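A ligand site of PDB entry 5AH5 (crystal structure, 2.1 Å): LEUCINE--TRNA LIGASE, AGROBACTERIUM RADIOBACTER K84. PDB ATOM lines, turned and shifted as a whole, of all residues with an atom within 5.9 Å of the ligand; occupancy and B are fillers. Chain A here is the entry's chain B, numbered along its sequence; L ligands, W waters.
The side-chain hydroxyl (OH) of Tyr 523 is in hydrogen-bond range of a ring nitrogen (NE2) of His 533 (2.6 Å). The backbone NH (N) of His 47 lies within hydrogen-bond range of a ring nitrogen (ND1) of His 50 (3.1 Å). N of Phe 39 sits at hydrogen-bond distance from OH of Tyr 496 (3.4 Å). The side-chain hydroxyl (OH) of Tyr 523 is in hydrogen-bond range of the side-chain hydroxyl (OH) of Tyr 496, 2.6 Å away. The backbone carbonyl oxygen (O) of Gly 563 sits at hydrogen-bond distance from the guanidinium group (NH1) of Arg 52 (2.8 Å). The backbone carbonyl oxygen of Ser 493 lies close to a ring nitrogen (ND1) of His 533, 3.0 Å away. N of Met 38 lies within hydrogen-bond range of O of Ile 524, 3.0 Å away. SD of Met 38 lies within hydrogen-bond range of N of Gly 526 (3.7 Å).
A nitrogen (N2) of the ligand sits close to the backbone NH (N) of Tyr 41, at 3.3 Å. O of Val 565 lies within hydrogen-bond range of N5 of the ligand, at 3.1 Å. The backbone NH (N) of Gly 526 is in hydrogen-bond range of an oxygen (O3) of the ligand, at 3.1 Å. The side-chain carboxylate (OD2) of Asp 78 lies within salt-bridge range of a nitrogen (N4) of the ligand, 2.6 Å away. N4 of the ligand sits at hydrogen-bond distance from O of Phe 39 (2.9 Å). The side-chain amide oxygen of Asn 53 is in hydrogen-bond range of an oxygen (O3) of the ligand (2.6 Å). N5 of the ligand is in hydrogen-bond range of SD of Met 564 (3.7 Å). A ring nitrogen (NE2) of His 47 lies within hydrogen-bond range of a nitrogen (N6) of the ligand (2.9 Å). The side-chain sulfur (SD) of Met 38 sits close to an oxygen (O3) of the ligand (3.7 Å). A ring nitrogen (NE2) of His 529 lies within hydrogen-bond range of an oxygen (O1) of the ligand (2.8 Å). O2 of the ligand sits at hydrogen-bond distance from OE2 of Glu 528 (2.6 Å). The side-chain amide nitrogen (NE2) of Gln 562 is in hydrogen-bond range of a nitrogen (N3) of the ligand, at 2.9 Å. A ring nitrogen (NE2) of His 50 sits at hydrogen-bond distance from an oxygen (O7) of the ligand, 2.9 Å away. A nitrogen (N1) of the ligand sits at hydrogen-bond distance from the backbone NH (N) of Val 565, 2.8 Å away.
Residues that only touch the ligand: Pro 40, Gly 49, Tyr 54, Ser 493, Tyr 496, Tyr 523, Gly 525, His 533 and Gly 563. Hydrophobic or aromatic side chains that line the ligand: Met 38, Phe 39, Pro 40, Tyr 41, His 47, His 50, Tyr 496, His 529, His 533, Met 564 and Val 565. Within 4 Å of the ligand: Met 38, Phe 39, Pro 40, Tyr 41, His 47, Gly 49, His 50, Asn 53, Tyr 54, Asp 78, Ser 493, Tyr 496, Tyr 523, Gly 525, Gly 526, Glu 528, His 529, His 533, Gln 562, Gly 563, Met 564 and Val 565.
Water W4 bridges OE2 of Glu 528 and O1 of the ligand. Water W5 bridges an oxygen (O6) of the ligand (3.1 Å) and a ring nitrogen (NE2) of His 47 (3.3 Å). Water W1 lies within hydrogen-bond range of N of Gly 49 (2.7 Å), N5 of the ligand (3.2 Å) and NE2 of His 47 (3.2 Å).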
ATOM      1  N   GLU A  37     -15.526 -29.098   2.881  1.00  0.00           N
ATOM      2  CA  GLU A  37     -15.151 -29.052   4.260  1.00  0.00           C
ATOM      3  C   GLU A  37     -16.416 -29.278   5.083  1.00  0.00           C
ATOM      4  O   GLU A  37     -17.559 -29.095   4.579  1.00  0.00           O
ATOM      5  CB  GLU A  37     -14.675 -27.669   4.635  1.00  0.00           C
ATOM      6  CG  GLU A  37     -13.515 -27.085   3.858  1.00  0.00           C
ATOM      7  CD  GLU A  37     -13.936 -26.120   2.814  1.00  0.00           C
ATOM      8  OE1 GLU A  37     -14.991 -25.464   3.004  1.00  0.00           O
ATOM      9  OE2 GLU A  37     -13.184 -25.963   1.802  1.00  0.00           O
ATOM     10  N   MET A  38     -16.227 -29.634   6.342  1.00  0.00           N
ATOM     11  CA  MET A  38     -17.373 -29.875   7.226  1.00  0.00           C
ATOM     12  C   MET A  38     -18.123 -28.596   7.484  1.00  0.00           C
ATOM     13  O   MET A  38     -17.594 -27.637   8.100  1.00  0.00           O
ATOM     14  CB  MET A  38     -16.973 -30.587   8.514  1.00  0.00           C
ATOM     15  CG  MET A  38     -16.604 -32.018   8.294  1.00  0.00           C
ATOM     16  SD  MET A  38     -16.152 -32.711   9.879  1.00  0.00           S
ATOM     17  CE  MET A  38     -15.339 -34.208   9.415  1.00  0.00           C
ATOM     18  N   PHE A  39     -19.347 -28.523   6.924  1.00  0.00           N
ATOM     19  CA  PHE A  39     -20.197 -27.297   7.025  1.00  0.00           C
ATOM     20  C   PHE A  39     -20.539 -26.942   8.474  1.00  0.00           C
ATOM     21  O   PHE A  39     -20.571 -27.807   9.317  1.00  0.00           O
ATOM     22  CB  PHE A  39     -21.387 -27.345   6.035  1.00  0.00           C
ATOM     23  CG  PHE A  39     -22.588 -28.224   6.420  1.00  0.00           C
ATOM     24  CD1 PHE A  39     -22.471 -29.405   7.131  1.00  0.00           C
ATOM     25  CD2 PHE A  39     -23.852 -27.904   5.913  1.00  0.00           C
ATOM     26  CE1 PHE A  39     -23.573 -30.168   7.390  1.00  0.00           C
ATOM     27  CE2 PHE A  39     -24.956 -28.686   6.185  1.00  0.00           C
ATOM     28  CZ  PHE A  39     -24.829 -29.829   6.891  1.00  0.00           C
ATOM     29  N   PRO A  40     -20.546 -25.670   8.820  1.00  0.00           N
ATOM     30  CA  PRO A  40     -20.630 -25.280  10.186  1.00  0.00           C
ATOM     31  C   PRO A  40     -22.070 -25.263  10.798  1.00  0.00           C
ATOM     32  O   PRO A  40     -23.032 -24.987  10.096  1.00  0.00           O
ATOM     33  CB  PRO A  40     -20.122 -23.878  10.167  1.00  0.00           C
ATOM     34  CG  PRO A  40     -20.517 -23.364   8.885  1.00  0.00           C
ATOM     35  CD  PRO A  40     -20.435 -24.518   7.944  1.00  0.00           C
ATOM     36  N   TYR A  41     -22.170 -25.481  12.111  1.00  0.00           N
ATOM     37  CA  TYR A  41     -23.447 -25.245  12.845  1.00  0.00           C
ATOM     38  C   TYR A  41     -23.720 -23.767  12.882  1.00  0.00           C
ATOM     39  O   TYR A  41     -22.849 -22.933  13.139  1.00  0.00           O
ATOM     40  CB  TYR A  41     -23.401 -25.792  14.276  1.00  0.00           C
ATOM     41  CG  TYR A  41     -23.350 -27.329  14.365  1.00  0.00           C
ATOM     42  CD1 TYR A  41     -24.378 -28.102  13.806  1.00  0.00           C
ATOM     43  CD2 TYR A  41     -22.292 -28.006  14.995  1.00  0.00           C
ATOM     44  CE1 TYR A  41     -24.394 -29.452  13.916  1.00  0.00           C
ATOM     45  CE2 TYR A  41     -22.301 -29.422  15.085  1.00  0.00           C
ATOM     46  CZ  TYR A  41     -23.320 -30.117  14.510  1.00  0.00           C
ATOM     47  OH  TYR A  41     -23.358 -31.501  14.534  1.00  0.00           O
ATOM     48  N   SER A  43     -24.562 -21.702  15.126  1.00  0.00           N
ATOM     49  CA  SER A  43     -24.678 -21.456  16.538  1.00  0.00           C
ATOM     50  C   SER A  43     -24.012 -20.170  16.968  1.00  0.00           C
ATOM     51  O   SER A  43     -23.939 -19.887  18.151  1.00  0.00           O
ATOM     52  CB  SER A  43     -24.122 -22.617  17.294  1.00  0.00           C
ATOM     53  OG  SER A  43     -22.748 -22.876  16.958  1.00  0.00           O
ATOM     54  N   HIS A  47     -15.753 -18.510  13.736  1.00  0.00           N
ATOM     55  CA  HIS A  47     -14.574 -18.435  14.572  1.00  0.00           C
ATOM     56  C   HIS A  47     -13.269 -18.953  13.903  1.00  0.00           C
ATOM     57  O   HIS A  47     -13.285 -19.701  12.900  1.00  0.00           O
ATOM     58  CB  HIS A  47     -14.885 -19.046  15.948  1.00  0.00           C
ATOM     59  CG  HIS A  47     -14.976 -20.532  15.970  1.00  0.00           C
ATOM     60  ND1 HIS A  47     -15.480 -21.230  17.039  1.00  0.00           N
ATOM     61  CD2 HIS A  47     -14.574 -21.445  15.066  1.00  0.00           C
ATOM     62  CE1 HIS A  47     -15.376 -22.527  16.803  1.00  0.00           C
ATOM     63  NE2 HIS A  47     -14.853 -22.683  15.607  1.00  0.00           N
ATOM     64  N   ILE A  48     -12.136 -18.552  14.469  1.00  0.00           N
ATOM     65  CA  ILE A  48     -10.841 -18.696  13.861  1.00  0.00           C
ATOM     66  C   ILE A  48     -10.529 -20.103  13.437  1.00  0.00           C
ATOM     67  O   ILE A  48      -9.838 -20.335  12.438  1.00  0.00           O
ATOM     68  CB  ILE A  48      -9.699 -18.105  14.738  1.00  0.00           C
ATOM     69  CG1 ILE A  48      -8.463 -17.802  13.879  1.00  0.00           C
ATOM     70  CG2 ILE A  48      -9.448 -19.039  15.921  1.00  0.00           C
ATOM     71  CD1 ILE A  48      -8.543 -16.521  13.030  1.00  0.00           C
ATOM     72  N   GLY A  49     -11.062 -21.066  14.130  1.00  0.00           N
ATOM     73  CA  GLY A  49     -10.941 -22.445  13.768  1.00  0.00           C
ATOM     74  C   GLY A  49     -11.543 -22.788  12.442  1.00  0.00           C
ATOM     75  O   GLY A  49     -10.950 -23.562  11.657  1.00  0.00           O
ATOM     76  N   HIS A  50     -12.748 -22.237  12.180  1.00  0.00           N
ATOM     77  CA  HIS A  50     -13.331 -22.353  10.871  1.00  0.00           C
ATOM     78  C   HIS A  50     -12.437 -21.774   9.783  1.00  0.00           C
ATOM     79  O   HIS A  50     -12.436 -22.286   8.693  1.00  0.00           O
ATOM     80  CB  HIS A  50     -14.691 -21.592  10.798  1.00  0.00           C
ATOM     81  CG  HIS A  50     -15.748 -22.112  11.731  1.00  0.00           C
ATOM     82  ND1 HIS A  50     -16.492 -21.283  12.535  1.00  0.00           N
ATOM     83  CD2 HIS A  50     -16.275 -23.347  11.894  1.00  0.00           C
ATOM     84  CE1 HIS A  50     -17.409 -21.980  13.177  1.00  0.00           C
ATOM     85  NE2 HIS A  50     -17.281 -23.236  12.819  1.00  0.00           N
ATOM     86  N   ARG A  52      -9.358 -21.669   9.609  1.00  0.00           N
ATOM     87  CA  ARG A  52      -8.253 -22.600   9.313  1.00  0.00           C
ATOM     88  C   ARG A  52      -8.760 -23.743   8.419  1.00  0.00           C
ATOM     89  O   ARG A  52      -8.141 -24.084   7.391  1.00  0.00           O
ATOM     90  CB  ARG A  52      -7.619 -23.184  10.563  1.00  0.00           C
ATOM     91  CG  ARG A  52      -6.427 -24.062  10.210  1.00  0.00           C
ATOM     92  CD  ARG A  52      -5.874 -24.778  11.384  1.00  0.00           C
ATOM     93  NE  ARG A  52      -4.544 -25.291  11.092  1.00  0.00           N
ATOM     94  CZ  ARG A  52      -3.860 -26.075  11.901  1.00  0.00           C
ATOM     95  NH1 ARG A  52      -4.366 -26.379  13.120  1.00  0.00           N
ATOM     96  NH2 ARG A  52      -2.641 -26.525  11.523  1.00  0.00           N
ATOM     97  N   ASN A  53      -9.859 -24.330   8.857  1.00  0.00           N
ATOM     98  CA  ASN A  53     -10.497 -25.413   8.173  1.00  0.00           C
ATOM     99  C   ASN A  53     -10.861 -25.078   6.682  1.00  0.00           C
ATOM    100  O   ASN A  53     -10.626 -25.885   5.757  1.00  0.00           O
ATOM    101  CB  ASN A  53     -11.737 -25.784   8.973  1.00  0.00           C
ATOM    102  CG  ASN A  53     -12.334 -27.085   8.577  1.00  0.00           C
ATOM    103  OD1 ASN A  53     -13.103 -27.647   9.381  1.00  0.00           O
ATOM    104  ND2 ASN A  53     -12.064 -27.569   7.370  1.00  0.00           N
ATOM    105  N   TYR A  54     -11.288 -23.858   6.470  1.00  0.00           N
ATOM    106  CA  TYR A  54     -11.882 -23.454   5.215  1.00  0.00           C
ATOM    107  C   TYR A  54     -10.824 -22.829   4.288  1.00  0.00           C
ATOM    108  O   TYR A  54     -10.921 -22.870   3.061  1.00  0.00           O
ATOM    109  CB  TYR A  54     -13.127 -22.561   5.469  1.00  0.00           C
ATOM    110  CG  TYR A  54     -14.250 -23.221   6.312  1.00  0.00           C
ATOM    111  CD1 TYR A  54     -14.410 -24.582   6.337  1.00  0.00           C
ATOM    112  CD2 TYR A  54     -15.178 -22.475   7.044  1.00  0.00           C
ATOM    113  CE1 TYR A  54     -15.391 -25.201   7.056  1.00  0.00           C
ATOM    114  CE2 TYR A  54     -16.184 -23.112   7.813  1.00  0.00           C
ATOM    115  CZ  TYR A  54     -16.294 -24.446   7.834  1.00  0.00           C
ATOM    116  OH  TYR A  54     -17.298 -25.132   8.541  1.00  0.00           O
ATOM    117  N   ASP A  78     -25.351 -25.990   8.541  1.00  0.00           N
ATOM    118  CA  ASP A  78     -25.879 -27.059   9.413  1.00  0.00           C
ATOM    119  C   ASP A  78     -26.729 -26.335  10.509  1.00  0.00           C
ATOM    120  O   ASP A  78     -26.243 -26.002  11.566  1.00  0.00           O
ATOM    121  CB  ASP A  78     -24.721 -27.867   9.958  1.00  0.00           C
ATOM    122  CG  ASP A  78     -25.070 -29.294  10.329  1.00  0.00           C
ATOM    123  OD1 ASP A  78     -26.230 -29.700  10.196  1.00  0.00           O
ATOM    124  OD2 ASP A  78     -24.129 -30.058  10.734  1.00  0.00           O
ATOM    125  N   PHE A 490     -27.823 -34.934  12.958  1.00  0.00           N
ATOM    126  CA  PHE A 490     -26.969 -35.829  12.200  1.00  0.00           C
ATOM    127  C   PHE A 490     -27.656 -36.585  11.070  1.00  0.00           C
ATOM    128  O   PHE A 490     -26.982 -37.125  10.159  1.00  0.00           O
ATOM    129  CB  PHE A 490     -26.173 -36.766  13.119  1.00  0.00           C
ATOM    130  CG  PHE A 490     -25.164 -36.031  13.934  1.00  0.00           C
ATOM    131  CD1 PHE A 490     -23.944 -35.620  13.344  1.00  0.00           C
ATOM    132  CD2 PHE A 490     -25.382 -35.743  15.279  1.00  0.00           C
ATOM    133  CE1 PHE A 490     -22.976 -35.005  14.103  1.00  0.00           C
ATOM    134  CE2 PHE A 490     -24.441 -35.070  16.032  1.00  0.00           C
ATOM    135  CZ  PHE A 490     -23.228 -34.678  15.435  1.00  0.00           C
ATOM    136  N   SER A 493     -27.015 -33.906   8.224  1.00  0.00           N
ATOM    137  CA  SER A 493     -25.663 -33.846   7.799  1.00  0.00           C
ATOM    138  C   SER A 493     -25.158 -35.190   7.299  1.00  0.00           C
ATOM    139  O   SER A 493     -24.044 -35.250   6.893  1.00  0.00           O
ATOM    140  CB  SER A 493     -24.799 -33.272   8.951  1.00  0.00           C
ATOM    141  OG  SER A 493     -24.860 -34.059  10.130  1.00  0.00           O
ATOM    142  N   TYR A 496     -25.930 -34.353   3.213  1.00  0.00           N
ATOM    143  CA  TYR A 496     -25.957 -32.997   2.605  1.00  0.00           C
ATOM    144  C   TYR A 496     -25.039 -32.781   1.412  1.00  0.00           C
ATOM    145  O   TYR A 496     -25.286 -31.904   0.562  1.00  0.00           O
ATOM    146  CB  TYR A 496     -25.606 -31.948   3.671  1.00  0.00           C
ATOM    147  CG  TYR A 496     -24.111 -31.811   4.076  1.00  0.00           C
ATOM    148  CD1 TYR A 496     -23.495 -32.743   4.878  1.00  0.00           C
ATOM    149  CD2 TYR A 496     -23.363 -30.715   3.682  1.00  0.00           C
ATOM    150  CE1 TYR A 496     -22.166 -32.613   5.277  1.00  0.00           C
ATOM    151  CE2 TYR A 496     -22.026 -30.557   4.077  1.00  0.00           C
ATOM    152  CZ  TYR A 496     -21.424 -31.500   4.842  1.00  0.00           C
ATOM    153  OH  TYR A 496     -20.109 -31.368   5.223  1.00  0.00           O
ATOM    154  N   TYR A 523     -12.281 -34.252   1.554  1.00  0.00           N
ATOM    155  CA  TYR A 523     -13.111 -33.782   2.655  1.00  0.00           C
ATOM    156  C   TYR A 523     -12.253 -33.369   3.846  1.00  0.00           C
ATOM    157  O   TYR A 523     -11.472 -34.164   4.338  1.00  0.00           O
ATOM    158  CB  TYR A 523     -14.020 -34.890   3.104  1.00  0.00           C
ATOM    159  CG  TYR A 523     -15.207 -34.456   3.952  1.00  0.00           C
ATOM    160  CD1 TYR A 523     -15.878 -33.244   3.724  1.00  0.00           C
ATOM    161  CD2 TYR A 523     -15.758 -35.316   4.864  1.00  0.00           C
ATOM    162  CE1 TYR A 523     -17.063 -32.900   4.440  1.00  0.00           C
ATOM    163  CE2 TYR A 523     -16.903 -34.946   5.619  1.00  0.00           C
ATOM    164  CZ  TYR A 523     -17.556 -33.731   5.376  1.00  0.00           C
ATOM    165  OH  TYR A 523     -18.730 -33.380   6.078  1.00  0.00           O
ATOM    166  N   ILE A 524     -12.406 -32.151   4.275  1.00  0.00           N
ATOM    167  CA  ILE A 524     -11.590 -31.554   5.335  1.00  0.00           C
ATOM    168  C   ILE A 524     -12.441 -31.253   6.552  1.00  0.00           C
ATOM    169  O   ILE A 524     -13.316 -30.408   6.468  1.00  0.00           O
ATOM    170  CB  ILE A 524     -11.014 -30.212   4.864  1.00  0.00           C
ATOM    171  CG1 ILE A 524     -10.422 -30.343   3.410  1.00  0.00           C
ATOM    172  CG2 ILE A 524      -9.932 -29.751   5.826  1.00  0.00           C
ATOM    173  CD1 ILE A 524     -10.130 -29.029   2.748  1.00  0.00           C
ATOM    174  N   GLY A 525     -12.176 -31.916   7.679  1.00  0.00           N
ATOM    175  CA  GLY A 525     -12.799 -31.538   8.934  1.00  0.00           C
ATOM    176  C   GLY A 525     -12.276 -32.282  10.149  1.00  0.00           C
ATOM    177  O   GLY A 525     -11.446 -33.171  10.030  1.00  0.00           O
ATOM    178  N   GLY A 526     -12.794 -31.934  11.304  1.00  0.00           N
ATOM    179  CA  GLY A 526     -12.237 -32.359  12.569  1.00  0.00           C
ATOM    180  C   GLY A 526     -12.477 -33.811  12.890  1.00  0.00           C
ATOM    181  O   GLY A 526     -13.474 -34.416  12.503  1.00  0.00           O
ATOM    182  N   ILE A 527     -11.516 -34.365  13.624  1.00  0.00           N
ATOM    183  CA  ILE A 527     -11.521 -35.734  14.044  1.00  0.00           C
ATOM    184  C   ILE A 527     -12.565 -35.972  15.107  1.00  0.00           C
ATOM    185  O   ILE A 527     -12.980 -37.128  15.319  1.00  0.00           O
ATOM    186  CB  ILE A 527     -10.103 -36.154  14.596  1.00  0.00           C
ATOM    187  CG1 ILE A 527     -10.016 -37.676  14.726  1.00  0.00           C
ATOM    188  CG2 ILE A 527      -9.788 -35.500  15.946  1.00  0.00           C
ATOM    189  CD1 ILE A 527      -8.605 -38.208  14.641  1.00  0.00           C
ATOM    190  N   GLU A 528     -12.994 -34.930  15.795  1.00  0.00           N
ATOM    191  CA  GLU A 528     -14.171 -35.100  16.685  1.00  0.00           C
ATOM    192  C   GLU A 528     -15.417 -35.812  16.048  1.00  0.00           C
ATOM    193  O   GLU A 528     -16.179 -36.459  16.771  1.00  0.00           O
ATOM    194  CB  GLU A 528     -14.576 -33.785  17.355  1.00  0.00           C
ATOM    195  CG  GLU A 528     -15.247 -32.798  16.441  1.00  0.00           C
ATOM    196  CD  GLU A 528     -14.275 -31.980  15.624  1.00  0.00           C
ATOM    197  OE1 GLU A 528     -13.030 -32.321  15.628  1.00  0.00           O
ATOM    198  OE2 GLU A 528     -14.773 -30.987  14.994  1.00  0.00           O
ATOM    199  N   HIS A 529     -15.559 -35.779  14.727  1.00  0.00           N
ATOM    200  CA  HIS A 529     -16.677 -36.459  14.043  1.00  0.00           C
ATOM    201  C   HIS A 529     -16.462 -37.916  13.679  1.00  0.00           C
ATOM    202  O   HIS A 529     -17.307 -38.541  13.033  1.00  0.00           O
ATOM    203  CB  HIS A 529     -17.146 -35.655  12.842  1.00  0.00           C
ATOM    204  CG  HIS A 529     -17.944 -34.472  13.232  1.00  0.00           C
ATOM    205  ND1 HIS A 529     -19.198 -34.589  13.850  1.00  0.00           N
ATOM    206  CD2 HIS A 529     -17.658 -33.156  13.205  1.00  0.00           C
ATOM    207  CE1 HIS A 529     -19.643 -33.382  14.121  1.00  0.00           C
ATOM    208  NE2 HIS A 529     -18.721 -32.497  13.770  1.00  0.00           N
ATOM    209  N   HIS A 533     -20.571 -37.814  12.560  1.00  0.00           N
ATOM    210  CA  HIS A 533     -20.930 -37.616  11.166  1.00  0.00           C
ATOM    211  C   HIS A 533     -20.180 -38.579  10.211  1.00  0.00           C
ATOM    212  O   HIS A 533     -20.786 -39.057   9.234  1.00  0.00           O
ATOM    213  CB  HIS A 533     -20.738 -36.145  10.806  1.00  0.00           C
ATOM    214  CG  HIS A 533     -20.546 -35.877   9.332  1.00  0.00           C
ATOM    215  ND1 HIS A 533     -21.579 -35.938   8.424  1.00  0.00           N
ATOM    216  CD2 HIS A 533     -19.467 -35.441   8.624  1.00  0.00           C
ATOM    217  CE1 HIS A 533     -21.137 -35.614   7.221  1.00  0.00           C
ATOM    218  NE2 HIS A 533     -19.845 -35.333   7.302  1.00  0.00           N
ATOM    219  N   GLN A 562      -7.938 -31.228   9.893  1.00  0.00           N
ATOM    220  CA  GLN A 562      -7.204 -30.071  10.362  1.00  0.00           C
ATOM    221  C   GLN A 562      -7.028 -30.109  11.903  1.00  0.00           C
ATOM    222  O   GLN A 562      -7.924 -30.539  12.643  1.00  0.00           O
ATOM    223  CB  GLN A 562      -7.773 -28.725   9.914  1.00  0.00           C
ATOM    224  CG  GLN A 562      -8.970 -28.143  10.758  1.00  0.00           C
ATOM    225  CD  GLN A 562     -10.156 -29.037  10.766  1.00  0.00           C
ATOM    226  OE1 GLN A 562     -10.269 -29.936   9.941  1.00  0.00           O
ATOM    227  NE2 GLN A 562     -11.069 -28.822  11.724  1.00  0.00           N
ATOM    228  N   GLY A 563      -5.883 -29.600  12.347  1.00  0.00           N
ATOM    229  CA  GLY A 563      -5.631 -29.422  13.765  1.00  0.00           C
ATOM    230  C   GLY A 563      -6.480 -28.352  14.422  1.00  0.00           C
ATOM    231  O   GLY A 563      -6.908 -27.369  13.784  1.00  0.00           O
ATOM    232  N   MET A 564      -6.683 -28.543  15.720  1.00  0.00           N
ATOM    233  CA  MET A 564      -7.257 -27.561  16.626  1.00  0.00           C
ATOM    234  C   MET A 564      -6.620 -26.167  16.572  1.00  0.00           C
ATOM    235  O   MET A 564      -5.367 -26.028  16.504  1.00  0.00           O
ATOM    236  CB  MET A 564      -7.057 -28.144  18.027  1.00  0.00           C
ATOM    237  CG  MET A 564      -7.760 -27.406  19.134  1.00  0.00           C
ATOM    238  SD  MET A 564      -9.546 -27.307  18.904  1.00  0.00           S
ATOM    239  CE  MET A 564      -9.868 -28.830  18.046  1.00  0.00           C
ATOM    240  N   VAL A 565      -7.446 -25.117  16.560  1.00  0.00           N
ATOM    241  CA  VAL A 565      -6.936 -23.832  16.887  1.00  0.00           C
ATOM    242  C   VAL A 565      -7.362 -23.488  18.318  1.00  0.00           C
ATOM    243  O   VAL A 565      -8.611 -23.433  18.627  1.00  0.00           O
ATOM    244  CB  VAL A 565      -7.370 -22.756  15.957  1.00  0.00           C
ATOM    245  CG1 VAL A 565      -6.617 -21.485  16.281  1.00  0.00           C
ATOM    246  CG2 VAL A 565      -7.125 -23.156  14.515  1.00  0.00           C
ATOM    247  N   ASN A 566      -6.350 -23.179  19.149  1.00  0.00           N
ATOM    248  CA  ASN A 566      -6.493 -22.933  20.580  1.00  0.00           C
ATOM    249  C   ASN A 566      -6.138 -21.502  20.809  1.00  0.00           C
ATOM    250  O   ASN A 566      -5.836 -20.746  19.845  1.00  0.00           O
ATOM    251  CB  ASN A 566      -5.538 -23.822  21.391  1.00  0.00           C
ATOM    252  CG  ASN A 566      -5.865 -25.286  21.311  1.00  0.00           C
ATOM    253  OD1 ASN A 566      -7.019 -25.708  21.509  1.00  0.00           O
ATOM    254  ND2 ASN A 566      -4.838 -26.077  21.051  1.00  0.00           N
ATOM    255  N   GLN A 573     -10.624 -22.624  22.758  1.00  0.00           N
ATOM    256  CA  GLN A 573     -11.345 -21.364  22.739  1.00  0.00           C
ATOM    257  C   GLN A 573     -12.791 -21.623  23.114  1.00  0.00           C
ATOM    258  O   GLN A 573     -13.370 -22.648  22.712  1.00  0.00           O
ATOM    259  CB  GLN A 573     -11.274 -20.683  21.395  1.00  0.00           C
ATOM    260  CG  GLN A 573      -9.826 -20.409  20.967  1.00  0.00           C
ATOM    261  CD  GLN A 573      -9.694 -19.262  20.013  1.00  0.00           C
ATOM    262  OE1 GLN A 573     -10.679 -18.678  19.564  1.00  0.00           O
ATOM    263  NE2 GLN A 573      -8.453 -18.918  19.701  1.00  0.00           N
HETATM  264  C1  LIG L   1     -19.766 -29.077  12.799  1.00  0.00           C
HETATM  265  N1  LIG L   1      -9.916 -25.519  15.250  1.00  0.00           N
HETATM  266  O1  LIG L   1     -18.949 -29.698  13.430  1.00  0.00           O
HETATM  267  S1  LIG L   1     -18.849 -26.907  13.530  1.00  0.00           S
HETATM  268  C2  LIG L   1      -9.965 -26.231  14.119  1.00  0.00           C
HETATM  269  N2  LIG L   1     -19.824 -27.760  12.773  1.00  0.00           N
HETATM  270  O2  LIG L   1     -13.658 -29.379  13.223  1.00  0.00           O
HETATM  271  N3  LIG L   1     -11.129 -26.574  13.529  1.00  0.00           N
HETATM  272  O3  LIG L   1     -14.562 -29.472  10.621  1.00  0.00           O
HETATM  273  C3  LIG L   1     -12.280 -26.172  14.098  1.00  0.00           C
HETATM  274  N4  LIG L   1     -21.941 -28.967  11.565  1.00  0.00           N
HETATM  275  O4  LIG L   1     -14.891 -26.393  11.751  1.00  0.00           O
HETATM  276  C4  LIG L   1     -12.298 -25.514  15.321  1.00  0.00           C
HETATM  277  O5  LIG L   1     -17.400 -27.177  12.916  1.00  0.00           O
HETATM  278  C5  LIG L   1     -11.081 -25.207  15.909  1.00  0.00           C
HETATM  279  N5  LIG L   1     -11.081 -24.509  17.075  1.00  0.00           N
HETATM  280  C6  LIG L   1     -21.112 -31.578  10.072  1.00  0.00           C
HETATM  281  N6  LIG L   1     -13.587 -25.299  15.666  1.00  0.00           N
HETATM  282  C7  LIG L   1     -14.374 -25.860  14.711  1.00  0.00           C
HETATM  283  C8  LIG L   1     -20.197 -30.641  10.874  1.00  0.00           C
HETATM  284  N7  LIG L   1     -13.566 -26.371  13.742  1.00  0.00           N
HETATM  285  C9  LIG L   1     -20.821 -29.826  12.029  1.00  0.00           C
HETATM  286  C10 LIG L   1     -21.537 -32.746  10.962  1.00  0.00           C
HETATM  287  C11 LIG L   1     -20.341 -31.992   8.767  1.00  0.00           C
HETATM  288  O6  LIG L   1     -18.665 -27.115  14.972  1.00  0.00           O
HETATM  289  C12 LIG L   1     -13.959 -27.099  12.551  1.00  0.00           C
HETATM  290  C13 LIG L   1     -14.595 -28.401  12.870  1.00  0.00           C
HETATM  291  C14 LIG L   1     -15.356 -28.736  11.588  1.00  0.00           C
HETATM  292  C15 LIG L   1     -15.718 -27.347  11.102  1.00  0.00           C
HETATM  293  C16 LIG L   1     -17.122 -26.922  11.542  1.00  0.00           C
HETATM  294  O7  LIG L   1     -19.039 -25.498  13.266  1.00  0.00           O
HETATM  295  O   HOH W   1     -12.024 -21.531  16.592  1.00  0.00           O
HETATM  296  O   HOH W   2     -19.841 -27.347  17.949  1.00  0.00           O
HETATM  297  O   HOH W   3     -13.168 -24.544  19.225  1.00  0.00           O
HETATM  298  O   HOH W   4     -17.042 -29.775  15.495  1.00  0.00           O
HETATM  299  O   HOH W   5     -17.434 -24.649  16.310  1.00  0.00           O
